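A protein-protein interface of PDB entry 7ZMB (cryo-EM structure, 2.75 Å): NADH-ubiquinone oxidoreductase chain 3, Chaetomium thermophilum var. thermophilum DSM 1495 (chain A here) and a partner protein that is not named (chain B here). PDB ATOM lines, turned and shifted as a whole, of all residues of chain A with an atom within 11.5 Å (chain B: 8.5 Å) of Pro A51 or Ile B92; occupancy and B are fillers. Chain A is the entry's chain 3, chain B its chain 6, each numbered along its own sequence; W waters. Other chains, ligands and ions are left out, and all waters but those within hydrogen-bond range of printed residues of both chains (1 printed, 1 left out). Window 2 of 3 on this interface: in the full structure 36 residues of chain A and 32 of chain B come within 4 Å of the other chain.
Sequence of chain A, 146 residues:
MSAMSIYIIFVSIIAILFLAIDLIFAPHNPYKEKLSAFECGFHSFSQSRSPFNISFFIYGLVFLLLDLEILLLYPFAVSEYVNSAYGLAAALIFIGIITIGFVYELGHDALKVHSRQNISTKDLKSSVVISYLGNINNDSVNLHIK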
ATOM      1  N   SER A  46     -22.817  -1.832  18.082  1.00  0.00           N
ATOM      2  CA  SER A  46     -22.366  -2.007  16.702  1.00  0.00           C
ATOM      3  C   SER A  46     -22.985  -3.293  16.171  1.00  0.00           C
ATOM      4  O   SER A  46     -22.550  -4.396  16.510  1.00  0.00           O
ATOM      5  CB  SER A  46     -20.846  -2.035  16.627  1.00  0.00           C
ATOM      6  OG  SER A  46     -20.416  -2.214  15.292  1.00  0.00           O
ATOM      7  N   GLN A  47     -24.025  -3.151  15.358  1.00  0.00           N
ATOM      8  CA  GLN A  47     -24.824  -4.279  14.899  1.00  0.00           C
ATOM      9  C   GLN A  47     -25.243  -4.135  13.442  1.00  0.00           C
ATOM     10  O   GLN A  47     -26.310  -4.596  13.047  1.00  0.00           O
ATOM     11  CB  GLN A  47     -26.004  -4.480  15.845  1.00  0.00           C
ATOM     12  CG  GLN A  47     -26.949  -3.336  15.859  1.00  0.00           C
ATOM     13  CD  GLN A  47     -28.064  -3.499  16.840  1.00  0.00           C
ATOM     14  OE1 GLN A  47     -28.197  -4.515  17.507  1.00  0.00           O
ATOM     15  NE2 GLN A  47     -28.810  -2.442  17.013  1.00  0.00           N
ATOM     16  N   SER A  48     -24.393  -3.511  12.631  1.00  0.00           N
ATOM     17  CA  SER A  48     -24.581  -3.403  11.191  1.00  0.00           C
ATOM     18  C   SER A  48     -23.928  -4.547  10.425  1.00  0.00           C
ATOM     19  O   SER A  48     -24.027  -4.588   9.197  1.00  0.00           O
ATOM     20  CB  SER A  48     -24.019  -2.070  10.688  1.00  0.00           C
ATOM     21  OG  SER A  48     -24.922  -1.004  10.907  1.00  0.00           O
ATOM     22  N   ARG A  49     -23.246  -5.453  11.113  1.00  0.00           N
ATOM     23  CA  ARG A  49     -22.615  -6.614  10.508  1.00  0.00           C
ATOM     24  C   ARG A  49     -23.233  -7.893  11.048  1.00  0.00           C
ATOM     25  O   ARG A  49     -22.551  -8.889  11.270  1.00  0.00           O
ATOM     26  CB  ARG A  49     -21.108  -6.597  10.737  1.00  0.00           C
ATOM     27  CG  ARG A  49     -20.404  -5.424  10.114  1.00  0.00           C
ATOM     28  CD  ARG A  49     -20.417  -5.567   8.615  1.00  0.00           C
ATOM     29  NE  ARG A  49     -19.688  -4.513   7.921  1.00  0.00           N
ATOM     30  CZ  ARG A  49     -20.250  -3.409   7.452  1.00  0.00           C
ATOM     31  NH1 ARG A  49     -21.546  -3.205   7.618  1.00  0.00           N
ATOM     32  NH2 ARG A  49     -19.517  -2.503   6.825  1.00  0.00           N
ATOM     33  N   SER A  50     -24.536  -7.861  11.279  1.00  0.00           N
ATOM     34  CA  SER A  50     -25.319  -8.992  11.745  1.00  0.00           C
ATOM     35  C   SER A  50     -26.588  -9.043  10.911  1.00  0.00           C
ATOM     36  O   SER A  50     -27.006  -8.026  10.352  1.00  0.00           O
ATOM     37  CB  SER A  50     -25.648  -8.870  13.239  1.00  0.00           C
ATOM     38  OG  SER A  50     -26.055  -7.559  13.566  1.00  0.00           O
ATOM     39  N   PRO A  51     -27.208 -10.218  10.786  1.00  0.00           N
ATOM     40  CA  PRO A  51     -28.333 -10.353   9.851  1.00  0.00           C
ATOM     41  C   PRO A  51     -29.457  -9.376  10.159  1.00  0.00           C
ATOM     42  O   PRO A  51     -29.775  -9.101  11.316  1.00  0.00           O
ATOM     43  CB  PRO A  51     -28.774 -11.809  10.039  1.00  0.00           C
ATOM     44  CG  PRO A  51     -27.540 -12.503  10.493  1.00  0.00           C
ATOM     45  CD  PRO A  51     -26.784 -11.517  11.332  1.00  0.00           C
ATOM     46  N   PHE A  52     -30.056  -8.845   9.099  1.00  0.00           N
ATOM     47  CA  PHE A  52     -31.011  -7.750   9.187  1.00  0.00           C
ATOM     48  C   PHE A  52     -32.210  -8.068   8.312  1.00  0.00           C
ATOM     49  O   PHE A  52     -32.052  -8.445   7.149  1.00  0.00           O
ATOM     50  CB  PHE A  52     -30.351  -6.437   8.752  1.00  0.00           C
ATOM     51  CG  PHE A  52     -31.238  -5.232   8.850  1.00  0.00           C
ATOM     52  CD1 PHE A  52     -31.420  -4.586  10.059  1.00  0.00           C
ATOM     53  CD2 PHE A  52     -31.855  -4.716   7.725  1.00  0.00           C
ATOM     54  CE1 PHE A  52     -32.220  -3.471  10.143  1.00  0.00           C
ATOM     55  CE2 PHE A  52     -32.654  -3.600   7.807  1.00  0.00           C
ATOM     56  CZ  PHE A  52     -32.834  -2.975   9.009  1.00  0.00           C
ATOM     57  N   ASN A  53     -33.401  -7.922   8.870  1.00  0.00           N
ATOM     58  CA  ASN A  53     -34.603  -8.210   8.106  1.00  0.00           C
ATOM     59  C   ASN A  53     -34.746  -7.251   6.936  1.00  0.00           C
ATOM     60  O   ASN A  53     -34.602  -6.037   7.087  1.00  0.00           O
ATOM     61  CB  ASN A  53     -35.839  -8.119   8.990  1.00  0.00           C
ATOM     62  CG  ASN A  53     -37.107  -8.328   8.213  1.00  0.00           C
ATOM     63  OD1 ASN A  53     -37.366  -9.417   7.709  1.00  0.00           O
ATOM     64  ND2 ASN A  53     -37.905  -7.276   8.094  1.00  0.00           N
ATOM     65  N   ILE A  54     -35.048  -7.802   5.771  1.00  0.00           N
ATOM     66  CA  ILE A  54     -35.398  -7.016   4.602  1.00  0.00           C
ATOM     67  C   ILE A  54     -36.829  -7.375   4.250  1.00  0.00           C
ATOM     68  O   ILE A  54     -37.121  -8.522   3.895  1.00  0.00           O
ATOM     69  CB  ILE A  54     -34.442  -7.258   3.430  1.00  0.00           C
ATOM     70  CG1 ILE A  54     -33.098  -6.596   3.738  1.00  0.00           C
ATOM     71  CG2 ILE A  54     -35.037  -6.715   2.138  1.00  0.00           C
ATOM     72  CD1 ILE A  54     -31.932  -7.217   3.051  1.00  0.00           C
ATOM     73  N   SER A  55     -37.722  -6.407   4.373  1.00  0.00           N
ATOM     74  CA  SER A  55     -39.139  -6.619   4.146  1.00  0.00           C
ATOM     75  C   SER A  55     -39.529  -6.522   2.680  1.00  0.00           C
ATOM     76  O   SER A  55     -40.711  -6.670   2.366  1.00  0.00           O
ATOM     77  CB  SER A  55     -39.947  -5.611   4.967  1.00  0.00           C
ATOM     78  OG  SER A  55     -39.490  -4.290   4.736  1.00  0.00           O
ATOM     79  N   LYS B  41     -12.521 -14.001   3.022  1.00  0.00           N
ATOM     80  CA  LYS B  41     -13.171 -14.312   4.288  1.00  0.00           C
ATOM     81  C   LYS B  41     -14.459 -13.525   4.480  1.00  0.00           C
ATOM     82  O   LYS B  41     -15.328 -13.952   5.245  1.00  0.00           O
ATOM     83  CB  LYS B  41     -12.198 -14.052   5.441  1.00  0.00           C
ATOM     84  CG  LYS B  41     -11.048 -15.049   5.466  1.00  0.00           C
ATOM     85  CD  LYS B  41      -9.991 -14.721   6.515  1.00  0.00           C
ATOM     86  CE  LYS B  41     -10.485 -14.955   7.929  1.00  0.00           C
ATOM     87  NZ  LYS B  41      -9.398 -14.739   8.923  1.00  0.00           N
ATOM     88  N   ASN B  42     -14.608 -12.408   3.793  1.00  0.00           N
ATOM     89  CA  ASN B  42     -15.793 -11.580   3.961  1.00  0.00           C
ATOM     90  C   ASN B  42     -16.740 -11.766   2.781  1.00  0.00           C
ATOM     91  O   ASN B  42     -16.307 -11.676   1.625  1.00  0.00           O
ATOM     92  CB  ASN B  42     -15.392 -10.115   4.103  1.00  0.00           C
ATOM     93  CG  ASN B  42     -16.572  -9.178   4.083  1.00  0.00           C
ATOM     94  OD1 ASN B  42     -16.838  -8.519   3.088  1.00  0.00           O
ATOM     95  ND2 ASN B  42     -17.307  -9.139   5.176  1.00  0.00           N
ATOM     96  N   PRO B  43     -18.021 -12.061   3.023  1.00  0.00           N
ATOM     97  CA  PRO B  43     -18.946 -12.349   1.914  1.00  0.00           C
ATOM     98  C   PRO B  43     -19.247 -11.166   1.018  1.00  0.00           C
ATOM     99  O   PRO B  43     -19.806 -11.368  -0.064  1.00  0.00           O
ATOM    100  CB  PRO B  43     -20.214 -12.818   2.635  1.00  0.00           C
ATOM    101  CG  PRO B  43     -19.739 -13.260   3.956  1.00  0.00           C
ATOM    102  CD  PRO B  43     -18.648 -12.331   4.322  1.00  0.00           C
ATOM    103  N   ILE B  44     -18.922  -9.946   1.426  1.00  0.00           N
ATOM    104  CA  ILE B  44     -19.201  -8.800   0.578  1.00  0.00           C
ATOM    105  C   ILE B  44     -18.040  -8.491  -0.366  1.00  0.00           C
ATOM    106  O   ILE B  44     -18.269  -8.077  -1.507  1.00  0.00           O
ATOM    107  CB  ILE B  44     -19.579  -7.585   1.438  1.00  0.00           C
ATOM    108  CG1 ILE B  44     -20.787  -7.926   2.309  1.00  0.00           C
ATOM    109  CG2 ILE B  44     -19.918  -6.399   0.579  1.00  0.00           C
ATOM    110  CD1 ILE B  44     -22.076  -8.049   1.555  1.00  0.00           C
ATOM    111  N   LEU B  84     -28.055 -10.480  -4.836  1.00  0.00           N
ATOM    112  CA  LEU B  84     -27.259 -11.396  -4.031  1.00  0.00           C
ATOM    113  C   LEU B  84     -26.652 -10.690  -2.828  1.00  0.00           C
ATOM    114  O   LEU B  84     -26.627 -11.242  -1.725  1.00  0.00           O
ATOM    115  CB  LEU B  84     -26.166 -12.012  -4.898  1.00  0.00           C
ATOM    116  CG  LEU B  84     -25.777 -13.461  -4.649  1.00  0.00           C
ATOM    117  CD1 LEU B  84     -27.003 -14.341  -4.662  1.00  0.00           C
ATOM    118  CD2 LEU B  84     -24.842 -13.866  -5.741  1.00  0.00           C
ATOM    119  N   PHE B  85     -26.147  -9.474  -3.033  1.00  0.00           N
ATOM    120  CA  PHE B  85     -25.740  -8.607  -1.935  1.00  0.00           C
ATOM    121  C   PHE B  85     -26.855  -8.494  -0.906  1.00  0.00           C
ATOM    122  O   PHE B  85     -26.634  -8.654   0.299  1.00  0.00           O
ATOM    123  CB  PHE B  85     -25.387  -7.233  -2.509  1.00  0.00           C
ATOM    124  CG  PHE B  85     -24.649  -6.326  -1.567  1.00  0.00           C
ATOM    125  CD1 PHE B  85     -25.289  -5.740  -0.491  1.00  0.00           C
ATOM    126  CD2 PHE B  85     -23.337  -5.995  -1.808  1.00  0.00           C
ATOM    127  CE1 PHE B  85     -24.617  -4.897   0.353  1.00  0.00           C
ATOM    128  CE2 PHE B  85     -22.669  -5.146  -0.972  1.00  0.00           C
ATOM    129  CZ  PHE B  85     -23.312  -4.598   0.116  1.00  0.00           C
ATOM    130  N   LEU B  86     -28.072  -8.238  -1.380  1.00  0.00           N
ATOM    131  CA  LEU B  86     -29.217  -8.049  -0.502  1.00  0.00           C
ATOM    132  C   LEU B  86     -29.495  -9.280   0.347  1.00  0.00           C
ATOM    133  O   LEU B  86     -29.956  -9.156   1.484  1.00  0.00           O
ATOM    134  CB  LEU B  86     -30.442  -7.689  -1.346  1.00  0.00           C
ATOM    135  CG  LEU B  86     -31.694  -7.160  -0.654  1.00  0.00           C
ATOM    136  CD1 LEU B  86     -31.613  -5.660  -0.474  1.00  0.00           C
ATOM    137  CD2 LEU B  86     -32.941  -7.553  -1.435  1.00  0.00           C
ATOM    138  N   PHE B  87     -29.238 -10.474  -0.180  1.00  0.00           N
ATOM    139  CA  PHE B  87     -29.517 -11.680   0.589  1.00  0.00           C
ATOM    140  C   PHE B  87     -28.408 -12.005   1.575  1.00  0.00           C
ATOM    141  O   PHE B  87     -28.681 -12.586   2.626  1.00  0.00           O
ATOM    142  CB  PHE B  87     -29.765 -12.851  -0.352  1.00  0.00           C
ATOM    143  CG  PHE B  87     -31.158 -12.902  -0.872  1.00  0.00           C
ATOM    144  CD1 PHE B  87     -31.533 -12.127  -1.949  1.00  0.00           C
ATOM    145  CD2 PHE B  87     -32.104 -13.716  -0.280  1.00  0.00           C
ATOM    146  CE1 PHE B  87     -32.812 -12.165  -2.427  1.00  0.00           C
ATOM    147  CE2 PHE B  87     -33.393 -13.750  -0.762  1.00  0.00           C
ATOM    148  CZ  PHE B  87     -33.744 -12.974  -1.830  1.00  0.00           C
ATOM    149  N   ILE B  88     -27.167 -11.627   1.268  1.00  0.00           N
ATOM    150  CA  ILE B  88     -26.078 -11.805   2.226  1.00  0.00           C
ATOM    151  C   ILE B  88     -26.323 -10.972   3.476  1.00  0.00           C
ATOM    152  O   ILE B  88     -26.056 -11.415   4.597  1.00  0.00           O
ATOM    153  CB  ILE B  88     -24.729 -11.463   1.574  1.00  0.00           C
ATOM    154  CG1 ILE B  88     -24.369 -12.504   0.516  1.00  0.00           C
ATOM    155  CG2 ILE B  88     -23.643 -11.377   2.621  1.00  0.00           C
ATOM    156  CD1 ILE B  88     -23.635 -11.940  -0.647  1.00  0.00           C
ATOM    157  N   LEU B  89     -26.839  -9.756   3.306  1.00  0.00           N
ATOM    158  CA  LEU B  89     -27.113  -8.900   4.455  1.00  0.00           C
ATOM    159  C   LEU B  89     -28.166  -9.517   5.361  1.00  0.00           C
ATOM    160  O   LEU B  89     -28.058  -9.447   6.588  1.00  0.00           O
ATOM    161  CB  LEU B  89     -27.561  -7.519   3.985  1.00  0.00           C
ATOM    162  CG  LEU B  89     -26.523  -6.679   3.254  1.00  0.00           C
ATOM    163  CD1 LEU B  89     -26.890  -5.213   3.297  1.00  0.00           C
ATOM    164  CD2 LEU B  89     -25.163  -6.913   3.845  1.00  0.00           C
ATOM    165  N   MET B  90     -29.193 -10.120   4.770  1.00  0.00           N
ATOM    166  CA  MET B  90     -30.303 -10.678   5.529  1.00  0.00           C
ATOM    167  C   MET B  90     -29.988 -12.039   6.143  1.00  0.00           C
ATOM    168  O   MET B  90     -30.471 -12.338   7.236  1.00  0.00           O
ATOM    169  CB  MET B  90     -31.527 -10.774   4.617  1.00  0.00           C
ATOM    170  CG  MET B  90     -32.746 -11.398   5.232  1.00  0.00           C
ATOM    171  SD  MET B  90     -34.194 -11.114   4.211  1.00  0.00           S
ATOM    172  CE  MET B  90     -33.737 -11.982   2.718  1.00  0.00           C
ATOM    173  N   LEU B  91     -29.184 -12.872   5.479  1.00  0.00           N
ATOM    174  CA  LEU B  91     -29.075 -14.282   5.837  1.00  0.00           C
ATOM    175  C   LEU B  91     -27.708 -14.706   6.349  1.00  0.00           C
ATOM    176  O   LEU B  91     -27.530 -15.884   6.681  1.00  0.00           O
ATOM    177  CB  LEU B  91     -29.431 -15.167   4.635  1.00  0.00           C
ATOM    178  CG  LEU B  91     -30.774 -14.964   3.946  1.00  0.00           C
ATOM    179  CD1 LEU B  91     -30.921 -15.944   2.801  1.00  0.00           C
ATOM    180  CD2 LEU B  91     -31.903 -15.115   4.933  1.00  0.00           C
ATOM    181  N   ILE B  92     -26.736 -13.809   6.409  1.00  0.00           N
ATOM    182  CA  ILE B  92     -25.388 -14.158   6.832  1.00  0.00           C
ATOM    183  C   ILE B  92     -24.978 -13.199   7.933  1.00  0.00           C
ATOM    184  O   ILE B  92     -25.203 -11.990   7.818  1.00  0.00           O
ATOM    185  CB  ILE B  92     -24.387 -14.101   5.660  1.00  0.00           C
ATOM    186  CG1 ILE B  92     -24.598 -15.277   4.714  1.00  0.00           C
ATOM    187  CG2 ILE B  92     -22.958 -14.097   6.159  1.00  0.00           C
ATOM    188  CD1 ILE B  92     -23.923 -15.102   3.384  1.00  0.00           C
ATOM    189  N   ASN B  93     -24.412 -13.735   9.006  1.00  0.00           N
ATOM    190  CA  ASN B  93     -23.709 -12.905   9.976  1.00  0.00           C
ATOM    191  C   ASN B  93     -22.337 -12.582   9.397  1.00  0.00           C
ATOM    192  O   ASN B  93     -21.482 -13.465   9.290  1.00  0.00           O
ATOM    193  CB  ASN B  93     -23.593 -13.608  11.323  1.00  0.00           C
ATOM    194  CG  ASN B  93     -23.411 -12.638  12.474  1.00  0.00           C
ATOM    195  OD1 ASN B  93     -22.510 -11.805  12.463  1.00  0.00           O
ATOM    196  ND2 ASN B  93     -24.257 -12.755  13.480  1.00  0.00           N
ATOM    197  N   ILE B  94     -22.134 -11.320   9.010  1.00  0.00           N
ATOM    198  CA  ILE B  94     -20.881 -10.921   8.374  1.00  0.00           C
ATOM    199  C   ILE B  94     -19.704 -11.132   9.313  1.00  0.00           C
ATOM    200  O   ILE B  94     -18.653 -11.638   8.905  1.00  0.00           O
ATOM    201  CB  ILE B  94     -20.957  -9.458   7.893  1.00  0.00           C
ATOM    202  CG1 ILE B  94     -21.868  -9.325   6.674  1.00  0.00           C
ATOM    203  CG2 ILE B  94     -19.568  -8.925   7.585  1.00  0.00           C
ATOM    204  CD1 ILE B  94     -21.341 -10.031   5.457  1.00  0.00           C
ATOM    205  N   ARG B  95     -19.846 -10.715  10.574  1.00  0.00           N
ATOM    206  CA  ARG B  95     -18.671 -10.772  11.490  1.00  0.00           C
ATOM    207  C   ARG B  95     -18.269 -12.223  11.752  1.00  0.00           C
ATOM    208  O   ARG B  95     -17.073 -12.522  11.604  1.00  0.00           O
ATOM    209  CB  ARG B  95     -18.882  -9.958  12.768  1.00  0.00           C
ATOM    210  CG  ARG B  95     -17.585  -9.558  13.457  1.00  0.00           C
ATOM    211  CD  ARG B  95     -17.830  -8.922  14.809  1.00  0.00           C
ATOM    212  NE  ARG B  95     -18.536  -9.833  15.698  1.00  0.00           N
ATOM    213  CZ  ARG B  95     -18.868  -9.551  16.951  1.00  0.00           C
ATOM    214  NH1 ARG B  95     -18.555  -8.377  17.471  1.00  0.00           N
ATOM    215  NH2 ARG B  95     -19.510 -10.446  17.680  1.00  0.00           N
ATOM    216  N   THR B  96     -19.228 -13.090  12.086  1.00  0.00           N
ATOM    217  CA  THR B  96     -18.871 -14.465  12.425  1.00  0.00           C
ATOM    218  C   THR B  96     -18.328 -15.208  11.210  1.00  0.00           C
ATOM    219  O   THR B  96     -17.541 -16.146  11.351  1.00  0.00           O
ATOM    220  CB  THR B  96     -20.069 -15.217  13.019  1.00  0.00           C
ATOM    221  OG1 THR B  96     -21.128 -15.289  12.065  1.00  0.00           O
ATOM    222  CG2 THR B  96     -20.587 -14.521  14.246  1.00  0.00           C
ATOM    223  N   SER B  97     -18.731 -14.799  10.009  1.00  0.00           N
ATOM    224  CA  SER B  97     -18.209 -15.438   8.806  1.00  0.00           C
ATOM    225  C   SER B  97     -16.794 -14.964   8.486  1.00  0.00           C
ATOM    226  O   SER B  97     -15.979 -15.735   7.971  1.00  0.00           O
ATOM    227  CB  SER B  97     -19.152 -15.194   7.629  1.00  0.00           C
ATOM    228  OG  SER B  97     -18.899 -13.955   7.014  1.00  0.00           O
ATOM    229  N   GLU B  98     -16.473 -13.705   8.780  1.00  0.00           N
ATOM    230  CA  GLU B  98     -15.086 -13.268   8.626  1.00  0.00           C
ATOM    231  C   GLU B  98     -14.157 -13.954   9.613  1.00  0.00           C
ATOM    232  O   GLU B  98     -12.936 -13.832   9.479  1.00  0.00           O
ATOM    233  CB  GLU B  98     -14.961 -11.758   8.797  1.00  0.00           C
ATOM    234  CG  GLU B  98     -15.517 -10.958   7.661  1.00  0.00           C
ATOM    235  CD  GLU B  98     -15.486  -9.472   7.943  1.00  0.00           C
ATOM    236  OE1 GLU B  98     -15.845  -9.072   9.072  1.00  0.00           O
ATOM    237  OE2 GLU B  98     -15.090  -8.705   7.040  1.00  0.00           O
ATOM    238  N   GLN B 100     -14.736 -17.250  10.047  1.00  0.00           N
ATOM    239  CA  GLN B 100     -14.971 -18.618   9.598  1.00  0.00           C
ATOM    240  C   GLN B 100     -13.756 -19.132   8.819  1.00  0.00           C
ATOM    241  O   GLN B 100     -13.828 -19.496   7.645  1.00  0.00           O
ATOM    242  CB  GLN B 100     -16.239 -18.648   8.756  1.00  0.00           C
ATOM    243  CG  GLN B 100     -17.003 -19.952   8.707  1.00  0.00           C
ATOM    244  CD  GLN B 100     -18.156 -19.875   7.724  1.00  0.00           C
ATOM    245  OE1 GLN B 100     -18.312 -18.877   7.026  1.00  0.00           O
ATOM    246  NE2 GLN B 100     -18.967 -20.919   7.671  1.00  0.00           N
HETATM  247  O   HOH W   1     -26.354  -7.029   7.448  1.00  0.00           O
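Water W1 bridges O of Leu B89 (3.1 Å) and O of Ser A50 (3.1 Å).
Pro A51 touches just these residues of chain B: Leu B89, Met B90, Ile B92 and Asn B93. Of the printed residues of chain A, Ile B92 touches Pro A51 (3.6 Å). Pro B43 touches none of the printed residues of chain A. No residue of chain A comes within 4 Å of Ile B88. Printed residues of chain A within 4 Å of Asn B93: Arg A49 (3.2 Å) and Pro A51 (3.5 Å). Ile B94 touches one residue of chain A. Of the printed residues of chain B, Arg A49 touches Asn B93 (3.2 Å), Ile B94 (3.3 Å) and Arg B95 (3.3 Å). Printed residues of chain A within 4 Å of Met B90: Pro A51, Phe A52 and Ile A54. Printed residues of chain B within 4 Å of Phe A52: Leu B89 (3.3 Å) and Met B90 (3.3 Å). The nearest residue of chain A that does not touch Ile B92 is Ser A50 (4.5 Å).
Pro A51 touches Leu B89 (CA to O, 3.4 Å). Pro A51 touches Met B90 (CB to O, 3.3 Å). Ile B92 touches Pro A51 (O to CG, 3.6 Å). Asn B93 touches Pro A51 (ND2 to CD, 3.5 Å). O of Phe A52 touches CA of Met B90 (3.3 Å). CD1 of Ile A54 touches O of Leu B86, at 3.2 Å.
The backbone NH (N) of Arg B95 lies close to the side-chain amide oxygen (OD1) of Asn B93 (3.4 Å). The backbone carbonyl oxygen (O) of Asn B93 lies close to the side-chain hydroxyl (OG1) of Thr B96, 3.3 Å away. The side-chain hydroxyl (OG) of Ser B97 sits close to the backbone carbonyl oxygen (O) of Asn B93. The backbone carbonyl oxygen (O) of Ile B94 sits at hydrogen-bond distance from the side-chain hydroxyl (OG) of Ser B97 (3.0 Å).
Printed residues of chain B that touch a printed residue of chain A: Leu B86, Leu B89, Met B90, Ile B92, Asn B93, Ile B94 and Arg B95. Along chain B the printed residues that touch a printed residue of chain A span positions 86 to 95. Among the printed residues, 11 pairs touch across the chains. Among the printed residues, no Asp or Glu carboxylate lies within 4 Å of a Lys or Arg side-chain nitrogen of the other chain.
O of Arg A49 sits close to OD1 of Asn B93. The backbone carbonyl oxygen (O) of Arg A49 sits at hydrogen-bond distance from the backbone NH (N) of Ile B94 (3.3 Å). The backbone carbonyl oxygen (O) of Arg A49 is in hydrogen-bond range of the backbone NH (N) of Arg B95, at 3.3 Å. O of Leu B89 sits at hydrogen-bond distance from N of Phe A52 (3.3 Å). N of Ile A54 lies within hydrogen-bond range of SD of Met B90 (3.8 Å).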
